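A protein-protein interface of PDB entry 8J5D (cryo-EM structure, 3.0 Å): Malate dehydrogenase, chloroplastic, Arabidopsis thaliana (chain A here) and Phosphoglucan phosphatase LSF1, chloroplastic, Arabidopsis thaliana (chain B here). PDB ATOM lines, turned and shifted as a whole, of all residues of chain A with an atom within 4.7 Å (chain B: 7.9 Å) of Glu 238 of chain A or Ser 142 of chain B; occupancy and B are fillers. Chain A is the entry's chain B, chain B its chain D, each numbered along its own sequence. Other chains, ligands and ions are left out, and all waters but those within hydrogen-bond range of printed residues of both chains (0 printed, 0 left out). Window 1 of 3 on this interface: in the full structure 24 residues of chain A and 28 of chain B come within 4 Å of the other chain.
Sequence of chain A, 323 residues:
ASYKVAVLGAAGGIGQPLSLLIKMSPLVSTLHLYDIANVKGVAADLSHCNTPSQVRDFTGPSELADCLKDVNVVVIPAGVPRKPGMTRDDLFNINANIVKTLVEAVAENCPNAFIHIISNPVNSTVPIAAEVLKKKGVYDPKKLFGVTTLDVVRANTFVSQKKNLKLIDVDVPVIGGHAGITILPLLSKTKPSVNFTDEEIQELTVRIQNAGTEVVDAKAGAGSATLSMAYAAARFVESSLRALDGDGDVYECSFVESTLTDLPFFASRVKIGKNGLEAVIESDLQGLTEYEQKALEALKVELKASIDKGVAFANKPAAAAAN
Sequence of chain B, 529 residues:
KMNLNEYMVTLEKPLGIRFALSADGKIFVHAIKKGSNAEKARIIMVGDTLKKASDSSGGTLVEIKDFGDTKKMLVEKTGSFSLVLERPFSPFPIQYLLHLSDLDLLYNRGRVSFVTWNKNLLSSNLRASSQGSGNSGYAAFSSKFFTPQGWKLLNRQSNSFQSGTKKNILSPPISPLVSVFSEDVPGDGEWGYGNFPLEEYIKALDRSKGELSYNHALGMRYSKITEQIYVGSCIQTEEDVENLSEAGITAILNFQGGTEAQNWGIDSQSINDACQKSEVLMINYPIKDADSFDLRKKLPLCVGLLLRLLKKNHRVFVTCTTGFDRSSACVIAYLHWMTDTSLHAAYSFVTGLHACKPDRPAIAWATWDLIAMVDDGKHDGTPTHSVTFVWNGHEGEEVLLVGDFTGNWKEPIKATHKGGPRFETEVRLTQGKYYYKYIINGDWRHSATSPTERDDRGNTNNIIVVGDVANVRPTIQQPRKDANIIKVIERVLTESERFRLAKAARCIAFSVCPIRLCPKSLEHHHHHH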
ATOM      1  N   LEU A  27     -19.340  -3.144  -6.478  1.00  0.00           N
ATOM      2  CA  LEU A  27     -18.044  -2.527  -6.225  1.00  0.00           C
ATOM      3  C   LEU A  27     -18.109  -1.378  -5.229  1.00  0.00           C
ATOM      4  O   LEU A  27     -17.170  -1.190  -4.451  1.00  0.00           O
ATOM      5  CB  LEU A  27     -17.438  -2.028  -7.539  1.00  0.00           C
ATOM      6  CG  LEU A  27     -17.063  -3.122  -8.538  1.00  0.00           C
ATOM      7  CD1 LEU A  27     -17.051  -2.581  -9.954  1.00  0.00           C
ATOM      8  CD2 LEU A  27     -15.714  -3.721  -8.180  1.00  0.00           C
ATOM      9  N   ALA A 234     -23.897   5.106 -14.613  1.00  0.00           N
ATOM     10  CA  ALA A 234     -23.603   3.955 -13.768  1.00  0.00           C
ATOM     11  C   ALA A 234     -22.661   2.985 -14.471  1.00  0.00           C
ATOM     12  O   ALA A 234     -21.775   2.402 -13.835  1.00  0.00           O
ATOM     13  CB  ALA A 234     -24.897   3.254 -13.366  1.00  0.00           C
ATOM     14  N   ARG A 235     -22.835   2.801 -15.783  1.00  0.00           N
ATOM     15  CA  ARG A 235     -21.903   1.966 -16.536  1.00  0.00           C
ATOM     16  C   ARG A 235     -20.487   2.526 -16.475  1.00  0.00           C
ATOM     17  O   ARG A 235     -19.521   1.780 -16.269  1.00  0.00           O
ATOM     18  CB  ARG A 235     -22.360   1.841 -17.987  1.00  0.00           C
ATOM     19  CG  ARG A 235     -21.342   1.173 -18.890  1.00  0.00           C
ATOM     20  CD  ARG A 235     -21.742   1.260 -20.351  1.00  0.00           C
ATOM     21  NE  ARG A 235     -20.590   1.111 -21.231  1.00  0.00           N
ATOM     22  CZ  ARG A 235     -20.651   0.671 -22.481  1.00  0.00           C
ATOM     23  NH1 ARG A 235     -21.800   0.331 -23.039  1.00  0.00           N
ATOM     24  NH2 ARG A 235     -19.530   0.571 -23.187  1.00  0.00           N
ATOM     25  N   PHE A 236     -20.347   3.841 -16.654  1.00  0.00           N
ATOM     26  CA  PHE A 236     -19.029   4.464 -16.591  1.00  0.00           C
ATOM     27  C   PHE A 236     -18.426   4.352 -15.196  1.00  0.00           C
ATOM     28  O   PHE A 236     -17.221   4.123 -15.054  1.00  0.00           O
ATOM     29  CB  PHE A 236     -19.115   5.928 -17.020  1.00  0.00           C
ATOM     30  CG  PHE A 236     -17.791   6.523 -17.410  1.00  0.00           C
ATOM     31  CD1 PHE A 236     -17.016   5.935 -18.393  1.00  0.00           C
ATOM     32  CD2 PHE A 236     -17.324   7.672 -16.798  1.00  0.00           C
ATOM     33  CE1 PHE A 236     -15.801   6.479 -18.756  1.00  0.00           C
ATOM     34  CE2 PHE A 236     -16.111   8.219 -17.158  1.00  0.00           C
ATOM     35  CZ  PHE A 236     -15.350   7.622 -18.136  1.00  0.00           C
ATOM     36  N   VAL A 237     -19.245   4.519 -14.156  1.00  0.00           N
ATOM     37  CA  VAL A 237     -18.748   4.388 -12.789  1.00  0.00           C
ATOM     38  C   VAL A 237     -18.255   2.971 -12.536  1.00  0.00           C
ATOM     39  O   VAL A 237     -17.197   2.767 -11.928  1.00  0.00           O
ATOM     40  CB  VAL A 237     -19.836   4.796 -11.780  1.00  0.00           C
ATOM     41  CG1 VAL A 237     -19.413   4.433 -10.369  1.00  0.00           C
ATOM     42  CG2 VAL A 237     -20.110   6.279 -11.876  1.00  0.00           C
ATOM     43  N   GLU A 238     -19.010   1.970 -12.993  1.00  0.00           N
ATOM     44  CA  GLU A 238     -18.570   0.590 -12.819  1.00  0.00           C
ATOM     45  C   GLU A 238     -17.273   0.325 -13.571  1.00  0.00           C
ATOM     46  O   GLU A 238     -16.367  -0.332 -13.044  1.00  0.00           O
ATOM     47  CB  GLU A 238     -19.657  -0.379 -13.279  1.00  0.00           C
ATOM     48  CG  GLU A 238     -19.166  -1.810 -13.406  1.00  0.00           C
ATOM     49  CD  GLU A 238     -20.291  -2.807 -13.547  1.00  0.00           C
ATOM     50  OE1 GLU A 238     -21.330  -2.630 -12.878  1.00  0.00           O
ATOM     51  OE2 GLU A 238     -20.136  -3.769 -14.327  1.00  0.00           O
ATOM     52  N   SER A 239     -17.165   0.823 -14.807  1.00  0.00           N
ATOM     53  CA  SER A 239     -15.937   0.626 -15.572  1.00  0.00           C
ATOM     54  C   SER A 239     -14.745   1.271 -14.876  1.00  0.00           C
ATOM     55  O   SER A 239     -13.676   0.660 -14.767  1.00  0.00           O
ATOM     56  CB  SER A 239     -16.098   1.188 -16.984  1.00  0.00           C
ATOM     57  OG  SER A 239     -16.887   0.329 -17.787  1.00  0.00           O
ATOM     58  N   SER A 240     -14.913   2.500 -14.387  1.00  0.00           N
ATOM     59  CA  SER A 240     -13.819   3.175 -13.697  1.00  0.00           C
ATOM     60  C   SER A 240     -13.433   2.441 -12.421  1.00  0.00           C
ATOM     61  O   SER A 240     -12.245   2.306 -12.111  1.00  0.00           O
ATOM     62  CB  SER A 240     -14.205   4.620 -13.390  1.00  0.00           C
ATOM     63  OG  SER A 240     -14.235   5.396 -14.574  1.00  0.00           O
ATOM     64  N   LEU A 241     -14.422   1.955 -11.667  1.00  0.00           N
ATOM     65  CA  LEU A 241     -14.119   1.250 -10.426  1.00  0.00           C
ATOM     66  C   LEU A 241     -13.394  -0.063 -10.690  1.00  0.00           C
ATOM     67  O   LEU A 241     -12.437  -0.400  -9.982  1.00  0.00           O
ATOM     68  CB  LEU A 241     -15.401   1.002  -9.638  1.00  0.00           C
ATOM     69  CG  LEU A 241     -15.955   2.227  -8.916  1.00  0.00           C
ATOM     70  CD1 LEU A 241     -17.166   1.844  -8.101  1.00  0.00           C
ATOM     71  CD2 LEU A 241     -14.892   2.846  -8.037  1.00  0.00           C
ATOM     72  N   ARG A 242     -13.823  -0.820 -11.702  1.00  0.00           N
ATOM     73  CA  ARG A 242     -13.148  -2.083 -11.976  1.00  0.00           C
ATOM     74  C   ARG A 242     -11.771  -1.859 -12.586  1.00  0.00           C
ATOM     75  O   ARG A 242     -10.870  -2.681 -12.388  1.00  0.00           O
ATOM     76  CB  ARG A 242     -14.009  -2.970 -12.877  1.00  0.00           C
ATOM     77  CG  ARG A 242     -14.324  -2.395 -14.236  1.00  0.00           C
ATOM     78  CD  ARG A 242     -15.410  -3.203 -14.922  1.00  0.00           C
ATOM     79  NE  ARG A 242     -14.902  -4.469 -15.432  1.00  0.00           N
ATOM     80  CZ  ARG A 242     -14.460  -4.652 -16.668  1.00  0.00           C
ATOM     81  NH1 ARG A 242     -14.463  -3.672 -17.556  1.00  0.00           N
ATOM     82  NH2 ARG A 242     -14.003  -5.851 -17.022  1.00  0.00           N
ATOM     83  N   TYR B 107     -16.258 -10.710 -23.448  1.00  0.00           N
ATOM     84  CA  TYR B 107     -17.576 -11.335 -23.463  1.00  0.00           C
ATOM     85  C   TYR B 107     -18.682 -10.288 -23.534  1.00  0.00           C
ATOM     86  O   TYR B 107     -19.472 -10.270 -24.483  1.00  0.00           O
ATOM     87  CB  TYR B 107     -17.749 -12.224 -22.228  1.00  0.00           C
ATOM     88  CG  TYR B 107     -19.045 -12.997 -22.210  1.00  0.00           C
ATOM     89  CD1 TYR B 107     -19.448 -13.740 -23.309  1.00  0.00           C
ATOM     90  CD2 TYR B 107     -19.869 -12.978 -21.094  1.00  0.00           C
ATOM     91  CE1 TYR B 107     -20.634 -14.444 -23.295  1.00  0.00           C
ATOM     92  CE2 TYR B 107     -21.053 -13.676 -21.072  1.00  0.00           C
ATOM     93  CZ  TYR B 107     -21.432 -14.408 -22.173  1.00  0.00           C
ATOM     94  OH  TYR B 107     -22.615 -15.107 -22.150  1.00  0.00           O
ATOM     95  N   ASN B 108     -18.744  -9.404 -22.541  1.00  0.00           N
ATOM     96  CA  ASN B 108     -19.683  -8.286 -22.561  1.00  0.00           C
ATOM     97  C   ASN B 108     -18.965  -7.095 -23.180  1.00  0.00           C
ATOM     98  O   ASN B 108     -18.415  -6.241 -22.485  1.00  0.00           O
ATOM     99  CB  ASN B 108     -20.194  -7.972 -21.161  1.00  0.00           C
ATOM    100  CG  ASN B 108     -21.691  -8.159 -21.035  1.00  0.00           C
ATOM    101  OD1 ASN B 108     -22.393  -8.319 -22.032  1.00  0.00           O
ATOM    102  ND2 ASN B 108     -22.189  -8.129 -19.806  1.00  0.00           N
ATOM    103  N   GLY B 110     -20.466  -4.761 -25.573  1.00  0.00           N
ATOM    104  CA  GLY B 110     -21.485  -3.807 -25.195  1.00  0.00           C
ATOM    105  C   GLY B 110     -22.001  -4.193 -23.826  1.00  0.00           C
ATOM    106  O   GLY B 110     -22.686  -5.209 -23.685  1.00  0.00           O
ATOM    107  N   ARG B 111     -21.684  -3.393 -22.809  1.00  0.00           N
ATOM    108  CA  ARG B 111     -21.877  -3.799 -21.418  1.00  0.00           C
ATOM    109  C   ARG B 111     -23.369  -3.801 -21.101  1.00  0.00           C
ATOM    110  O   ARG B 111     -23.914  -2.886 -20.479  1.00  0.00           O
ATOM    111  CB  ARG B 111     -21.104  -2.881 -20.482  1.00  0.00           C
ATOM    112  CG  ARG B 111     -19.608  -2.915 -20.705  1.00  0.00           C
ATOM    113  CD  ARG B 111     -19.017  -4.198 -20.160  1.00  0.00           C
ATOM    114  NE  ARG B 111     -17.564  -4.227 -20.267  1.00  0.00           N
ATOM    115  CZ  ARG B 111     -16.814  -5.271 -19.945  1.00  0.00           C
ATOM    116  NH1 ARG B 111     -17.347  -6.393 -19.490  1.00  0.00           N
ATOM    117  NH2 ARG B 111     -15.494  -5.188 -20.083  1.00  0.00           N
ATOM    118  N   VAL B 112     -24.038  -4.866 -21.551  1.00  0.00           N
ATOM    119  CA  VAL B 112     -25.461  -5.024 -21.293  1.00  0.00           C
ATOM    120  C   VAL B 112     -25.689  -5.132 -19.794  1.00  0.00           C
ATOM    121  O   VAL B 112     -25.001  -5.884 -19.092  1.00  0.00           O
ATOM    122  CB  VAL B 112     -25.996  -6.262 -22.032  1.00  0.00           C
ATOM    123  CG1 VAL B 112     -27.252  -6.794 -21.361  1.00  0.00           C
ATOM    124  CG2 VAL B 112     -26.240  -5.952 -23.496  1.00  0.00           C
ATOM    125  N   SER B 113     -26.652  -4.367 -19.291  1.00  0.00           N
ATOM    126  CA  SER B 113     -26.920  -4.367 -17.863  1.00  0.00           C
ATOM    127  C   SER B 113     -27.551  -5.682 -17.427  1.00  0.00           C
ATOM    128  O   SER B 113     -28.256  -6.348 -18.189  1.00  0.00           O
ATOM    129  CB  SER B 113     -27.837  -3.209 -17.484  1.00  0.00           C
ATOM    130  OG  SER B 113     -27.826  -2.993 -16.085  1.00  0.00           O
ATOM    131  N   PHE B 114     -27.289  -6.047 -16.177  1.00  0.00           N
ATOM    132  CA  PHE B 114     -27.838  -7.252 -15.569  1.00  0.00           C
ATOM    133  C   PHE B 114     -28.161  -6.906 -14.124  1.00  0.00           C
ATOM    134  O   PHE B 114     -27.252  -6.709 -13.312  1.00  0.00           O
ATOM    135  CB  PHE B 114     -26.850  -8.418 -15.660  1.00  0.00           C
ATOM    136  CG  PHE B 114     -27.433  -9.759 -15.282  1.00  0.00           C
ATOM    137  CD1 PHE B 114     -28.748  -9.882 -14.872  1.00  0.00           C
ATOM    138  CD2 PHE B 114     -26.651 -10.898 -15.336  1.00  0.00           C
ATOM    139  CE1 PHE B 114     -29.267 -11.111 -14.523  1.00  0.00           C
ATOM    140  CE2 PHE B 114     -27.167 -12.129 -14.991  1.00  0.00           C
ATOM    141  CZ  PHE B 114     -28.477 -12.234 -14.585  1.00  0.00           C
ATOM    142  N   TYR B 138     -28.158  -6.946  -7.411  1.00  0.00           N
ATOM    143  CA  TYR B 138     -27.062  -6.152  -7.935  1.00  0.00           C
ATOM    144  C   TYR B 138     -27.333  -5.797  -9.389  1.00  0.00           C
ATOM    145  O   TYR B 138     -27.896  -6.595 -10.148  1.00  0.00           O
ATOM    146  CB  TYR B 138     -25.729  -6.898  -7.824  1.00  0.00           C
ATOM    147  CG  TYR B 138     -25.279  -7.126  -6.402  1.00  0.00           C
ATOM    148  CD1 TYR B 138     -24.789  -6.080  -5.636  1.00  0.00           C
ATOM    149  CD2 TYR B 138     -25.341  -8.386  -5.828  1.00  0.00           C
ATOM    150  CE1 TYR B 138     -24.374  -6.280  -4.338  1.00  0.00           C
ATOM    151  CE2 TYR B 138     -24.930  -8.597  -4.528  1.00  0.00           C
ATOM    152  CZ  TYR B 138     -24.447  -7.540  -3.788  1.00  0.00           C
ATOM    153  OH  TYR B 138     -24.033  -7.741  -2.494  1.00  0.00           O
ATOM    154  N   ALA B 139     -26.943  -4.579  -9.754  1.00  0.00           N
ATOM    155  CA  ALA B 139     -26.981  -4.088 -11.127  1.00  0.00           C
ATOM    156  C   ALA B 139     -25.536  -3.984 -11.597  1.00  0.00           C
ATOM    157  O   ALA B 139     -24.798  -3.090 -11.171  1.00  0.00           O
ATOM    158  CB  ALA B 139     -27.695  -2.743 -11.211  1.00  0.00           C
ATOM    159  N   ALA B 140     -25.129  -4.899 -12.470  1.00  0.00           N
ATOM    160  CA  ALA B 140     -23.760  -4.951 -12.951  1.00  0.00           C
ATOM    161  C   ALA B 140     -23.740  -4.943 -14.472  1.00  0.00           C
ATOM    162  O   ALA B 140     -24.677  -5.407 -15.124  1.00  0.00           O
ATOM    163  CB  ALA B 140     -23.033  -6.192 -12.426  1.00  0.00           C
ATOM    164  N   PHE B 141     -22.659  -4.406 -15.029  1.00  0.00           N
ATOM    165  CA  PHE B 141     -22.479  -4.340 -16.471  1.00  0.00           C
ATOM    166  C   PHE B 141     -21.405  -5.283 -16.985  1.00  0.00           C
ATOM    167  O   PHE B 141     -21.548  -5.822 -18.084  1.00  0.00           O
ATOM    168  CB  PHE B 141     -22.138  -2.908 -16.898  1.00  0.00           C
ATOM    169  CG  PHE B 141     -23.222  -1.911 -16.594  1.00  0.00           C
ATOM    170  CD1 PHE B 141     -23.306  -1.316 -15.347  1.00  0.00           C
ATOM    171  CD2 PHE B 141     -24.157  -1.571 -17.555  1.00  0.00           C
ATOM    172  CE1 PHE B 141     -24.302  -0.405 -15.063  1.00  0.00           C
ATOM    173  CE2 PHE B 141     -25.154  -0.659 -17.277  1.00  0.00           C
ATOM    174  CZ  PHE B 141     -25.226  -0.075 -16.031  1.00  0.00           C
ATOM    175  N   SER B 142     -20.339  -5.496 -16.218  1.00  0.00           N
ATOM    176  CA  SER B 142     -19.335  -6.489 -16.568  1.00  0.00           C
ATOM    177  C   SER B 142     -19.832  -7.875 -16.185  1.00  0.00           C
ATOM    178  O   SER B 142     -20.339  -8.078 -15.078  1.00  0.00           O
ATOM    179  CB  SER B 142     -18.016  -6.186 -15.860  1.00  0.00           C
ATOM    180  OG  SER B 142     -18.188  -6.179 -14.455  1.00  0.00           O
ATOM    181  N   SER B 143     -19.681  -8.830 -17.098  1.00  0.00           N
ATOM    182  CA  SER B 143     -20.140 -10.194 -16.875  1.00  0.00           C
ATOM    183  C   SER B 143     -19.234 -10.983 -15.939  1.00  0.00           C
ATOM    184  O   SER B 143     -19.411 -12.198 -15.812  1.00  0.00           O
ATOM    185  CB  SER B 143     -20.269 -10.925 -18.212  1.00  0.00           C
ATOM    186  OG  SER B 143     -19.027 -10.955 -18.890  1.00  0.00           O
ATOM    187  N   LYS B 144     -18.274 -10.329 -15.288  1.00  0.00           N
ATOM    188  CA  LYS B 144     -17.391 -11.000 -14.345  1.00  0.00           C
ATOM    189  C   LYS B 144     -18.028 -11.215 -12.980  1.00  0.00           C
ATOM    190  O   LYS B 144     -17.481 -11.976 -12.175  1.00  0.00           O
ATOM    191  CB  LYS B 144     -16.098 -10.200 -14.179  1.00  0.00           C
ATOM    192  CG  LYS B 144     -16.168  -9.118 -13.116  1.00  0.00           C
ATOM    193  CD  LYS B 144     -14.789  -8.577 -12.787  1.00  0.00           C
ATOM    194  CE  LYS B 144     -14.829  -7.681 -11.562  1.00  0.00           C
ATOM    195  NZ  LYS B 144     -13.473  -7.237 -11.143  1.00  0.00           N
ATOM    196  N   PHE B 145     -19.161 -10.575 -12.702  1.00  0.00           N
ATOM    197  CA  PHE B 145     -19.817 -10.668 -11.406  1.00  0.00           C
ATOM    198  C   PHE B 145     -20.866 -11.767 -11.352  1.00  0.00           C
ATOM    199  O   PHE B 145     -21.581 -11.873 -10.351  1.00  0.00           O
ATOM    200  CB  PHE B 145     -20.465  -9.331 -11.048  1.00  0.00           C
ATOM    201  CG  PHE B 145     -19.482  -8.246 -10.718  1.00  0.00           C
ATOM    202  CD1 PHE B 145     -18.752  -8.288  -9.542  1.00  0.00           C
ATOM    203  CD2 PHE B 145     -19.297  -7.179 -11.579  1.00  0.00           C
ATOM    204  CE1 PHE B 145     -17.852  -7.288  -9.234  1.00  0.00           C
ATOM    205  CE2 PHE B 145     -18.398  -6.177 -11.276  1.00  0.00           C
ATOM    206  CZ  PHE B 145     -17.675  -6.232 -10.103  1.00  0.00           C
ATOM    207  N   PHE B 146     -20.981 -12.582 -12.397  1.00  0.00           N
ATOM    208  CA  PHE B 146     -22.048 -13.564 -12.500  1.00  0.00           C
ATOM    209  C   PHE B 146     -21.474 -14.939 -12.812  1.00  0.00           C
ATOM    210  O   PHE B 146     -20.326 -15.078 -13.239  1.00  0.00           O
ATOM    211  CB  PHE B 146     -23.068 -13.159 -13.571  1.00  0.00           C
ATOM    212  CG  PHE B 146     -23.646 -11.788 -13.363  1.00  0.00           C
ATOM    213  CD1 PHE B 146     -24.529 -11.546 -12.325  1.00  0.00           C
ATOM    214  CD2 PHE B 146     -23.298 -10.741 -14.198  1.00  0.00           C
ATOM    215  CE1 PHE B 146     -25.058 -10.288 -12.126  1.00  0.00           C
ATOM    216  CE2 PHE B 146     -23.823  -9.479 -14.003  1.00  0.00           C
ATOM    217  CZ  PHE B 146     -24.705  -9.253 -12.966  1.00  0.00           C
ATOM    218  N   TRP B 151     -24.401 -16.003 -17.326  1.00  0.00           N
ATOM    219  CA  TRP B 151     -23.966 -15.697 -18.687  1.00  0.00           C
ATOM    220  C   TRP B 151     -24.850 -16.391 -19.718  1.00  0.00           C
ATOM    221  O   TRP B 151     -25.174 -15.810 -20.762  1.00  0.00           O
ATOM    222  CB  TRP B 151     -22.502 -16.095 -18.876  1.00  0.00           C
ATOM    223  CG  TRP B 151     -21.582 -15.519 -17.843  1.00  0.00           C
ATOM    224  CD1 TRP B 151     -21.757 -14.361 -17.142  1.00  0.00           C
ATOM    225  CD2 TRP B 151     -20.336 -16.068 -17.403  1.00  0.00           C
ATOM    226  NE1 TRP B 151     -20.701 -14.161 -16.288  1.00  0.00           N
ATOM    227  CE2 TRP B 151     -19.814 -15.195 -16.430  1.00  0.00           C
ATOM    228  CE3 TRP B 151     -19.611 -17.215 -17.737  1.00  0.00           C
ATOM    229  CZ2 TRP B 151     -18.603 -15.433 -15.788  1.00  0.00           C
ATOM    230  CZ3 TRP B 151     -18.411 -17.451 -17.096  1.00  0.00           C
ATOM    231  CH2 TRP B 151     -17.918 -16.565 -16.133  1.00  0.00           C
ATOM    232  N   LEU B 154     -27.900 -14.477 -20.020  1.00  0.00           N
ATOM    233  CA  LEU B 154     -27.627 -13.303 -20.844  1.00  0.00           C
ATOM    234  C   LEU B 154     -27.675 -13.649 -22.327  1.00  0.00           C
ATOM    235  O   LEU B 154     -28.232 -12.892 -23.131  1.00  0.00           O
ATOM    236  CB  LEU B 154     -26.267 -12.708 -20.480  1.00  0.00           C
ATOM    237  CG  LEU B 154     -26.239 -11.631 -19.397  1.00  0.00           C
ATOM    238  CD1 LEU B 154     -24.823 -11.428 -18.885  1.00  0.00           C
ATOM    239  CD2 LEU B 154     -26.801 -10.330 -19.937  1.00  0.00           C
ATOM    240  N   VAL B 178     -14.394 -13.148 -19.954  1.00  0.00           N
ATOM    241  CA  VAL B 178     -15.275 -12.202 -19.281  1.00  0.00           C
ATOM    242  C   VAL B 178     -14.500 -11.205 -18.432  1.00  0.00           C
ATOM    243  O   VAL B 178     -15.026 -10.126 -18.127  1.00  0.00           O
ATOM    244  CB  VAL B 178     -16.319 -12.934 -18.422  1.00  0.00           C
ATOM    245  CG1 VAL B 178     -16.822 -14.171 -19.143  1.00  0.00           C
ATOM    246  CG2 VAL B 178     -15.746 -13.295 -17.060  1.00  0.00           C
ATOM    247  N   SER B 179     -13.267 -11.524 -18.044  1.00  0.00           N
ATOM    248  CA  SER B 179     -12.455 -10.566 -17.307  1.00  0.00           C
ATOM    249  C   SER B 179     -10.992 -10.969 -17.400  1.00  0.00           C
ATOM    250  O   SER B 179     -10.664 -12.132 -17.638  1.00  0.00           O
ATOM    251  CB  SER B 179     -12.888 -10.463 -15.842  1.00  0.00           C
ATOM    252  OG  SER B 179     -12.494 -11.608 -15.111  1.00  0.00           O
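The side-chain carboxylate (OE2) of Glu 238 of chain A lies within hydrogen-bond range of the backbone NH (N) of Ser 142 of chain B (2.6 Å). NH1 of Arg 242 of chain A lies close to NH2 of Arg 111 of chain B (3.1 Å). The backbone NH (N) of Phe 141 of chain B sits at hydrogen-bond distance from the side-chain carboxylate (OE2) of Glu 238 of chain A, 2.7 Å away.
The guanidinium group of Arg 111 of chain B is in hydrogen-bond range of the backbone carbonyl oxygen of Asn 108 of chain B (3.1 Å). N of Phe 114 of chain B lies within hydrogen-bond range of O of Ala 140 of chain B (2.9 Å). The side-chain amide nitrogen (ND2) of Asn 108 of chain B is in hydrogen-bond range of the backbone carbonyl oxygen (O) of Phe 141 of chain B (2.9 Å). The side-chain hydroxyl of Ser 239 of chain A is in hydrogen-bond range of the backbone carbonyl oxygen of Arg 235 of chain A, 3.4 Å away.
Leu 27 of chain A touches Phe 145 of chain B. Ala 234 of chain A touches Phe 141 of chain B (C to CE1, 3.8 Å). Arg 235 of chain A touches Arg 111 of chain B (NH1 to N, 3.7 Å). Phe 141 of chain B touches Arg 235 of chain A (CE1 to N, 3.6 Å). Glu 238 of chain A touches Ala 139 of chain B (OE1 to O, 3.9 Å). Glu 238 of chain A touches Ala 140 of chain B. NE of Arg 242 of chain A touches CB of Ser 142 of chain B (3.6 Å).
Of the printed residues of chain B, Ala 234 of chain A touches Phe 141 (3.8 Å). Of chain B, only Ala 139, Ala 140, Phe 141 and Ser 142 come within 4 Å of Glu 238 of chain A. Printed residues of chain B within 4 Å of Arg 242 of chain A: Arg 111 (3.1 Å) and Ser 142 (3.6 Å). Of the printed residues of chain A, Arg 111 of chain B touches Arg 235 (3.7 Å) and Arg 242 (3.1 Å). Printed residues of chain A within 4 Å of Ala 139 of chain B: Glu 238. Of the printed residues of chain A, Ala 140 of chain B touches Glu 238. Ser 142 of chain B touches just these residues of chain A: Glu 238 (2.6 Å) and Arg 242 (3.6 Å).
Printed residues of chain B that touch a printed residue of chain A: Arg 111, Ala 139, Ala 140, Phe 141, Ser 142 and Phe 145. Along chain B the printed residues that touch a printed residue of chain A span positions 111 to 145. Among the printed residues, 10 pairs touch across the chains.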
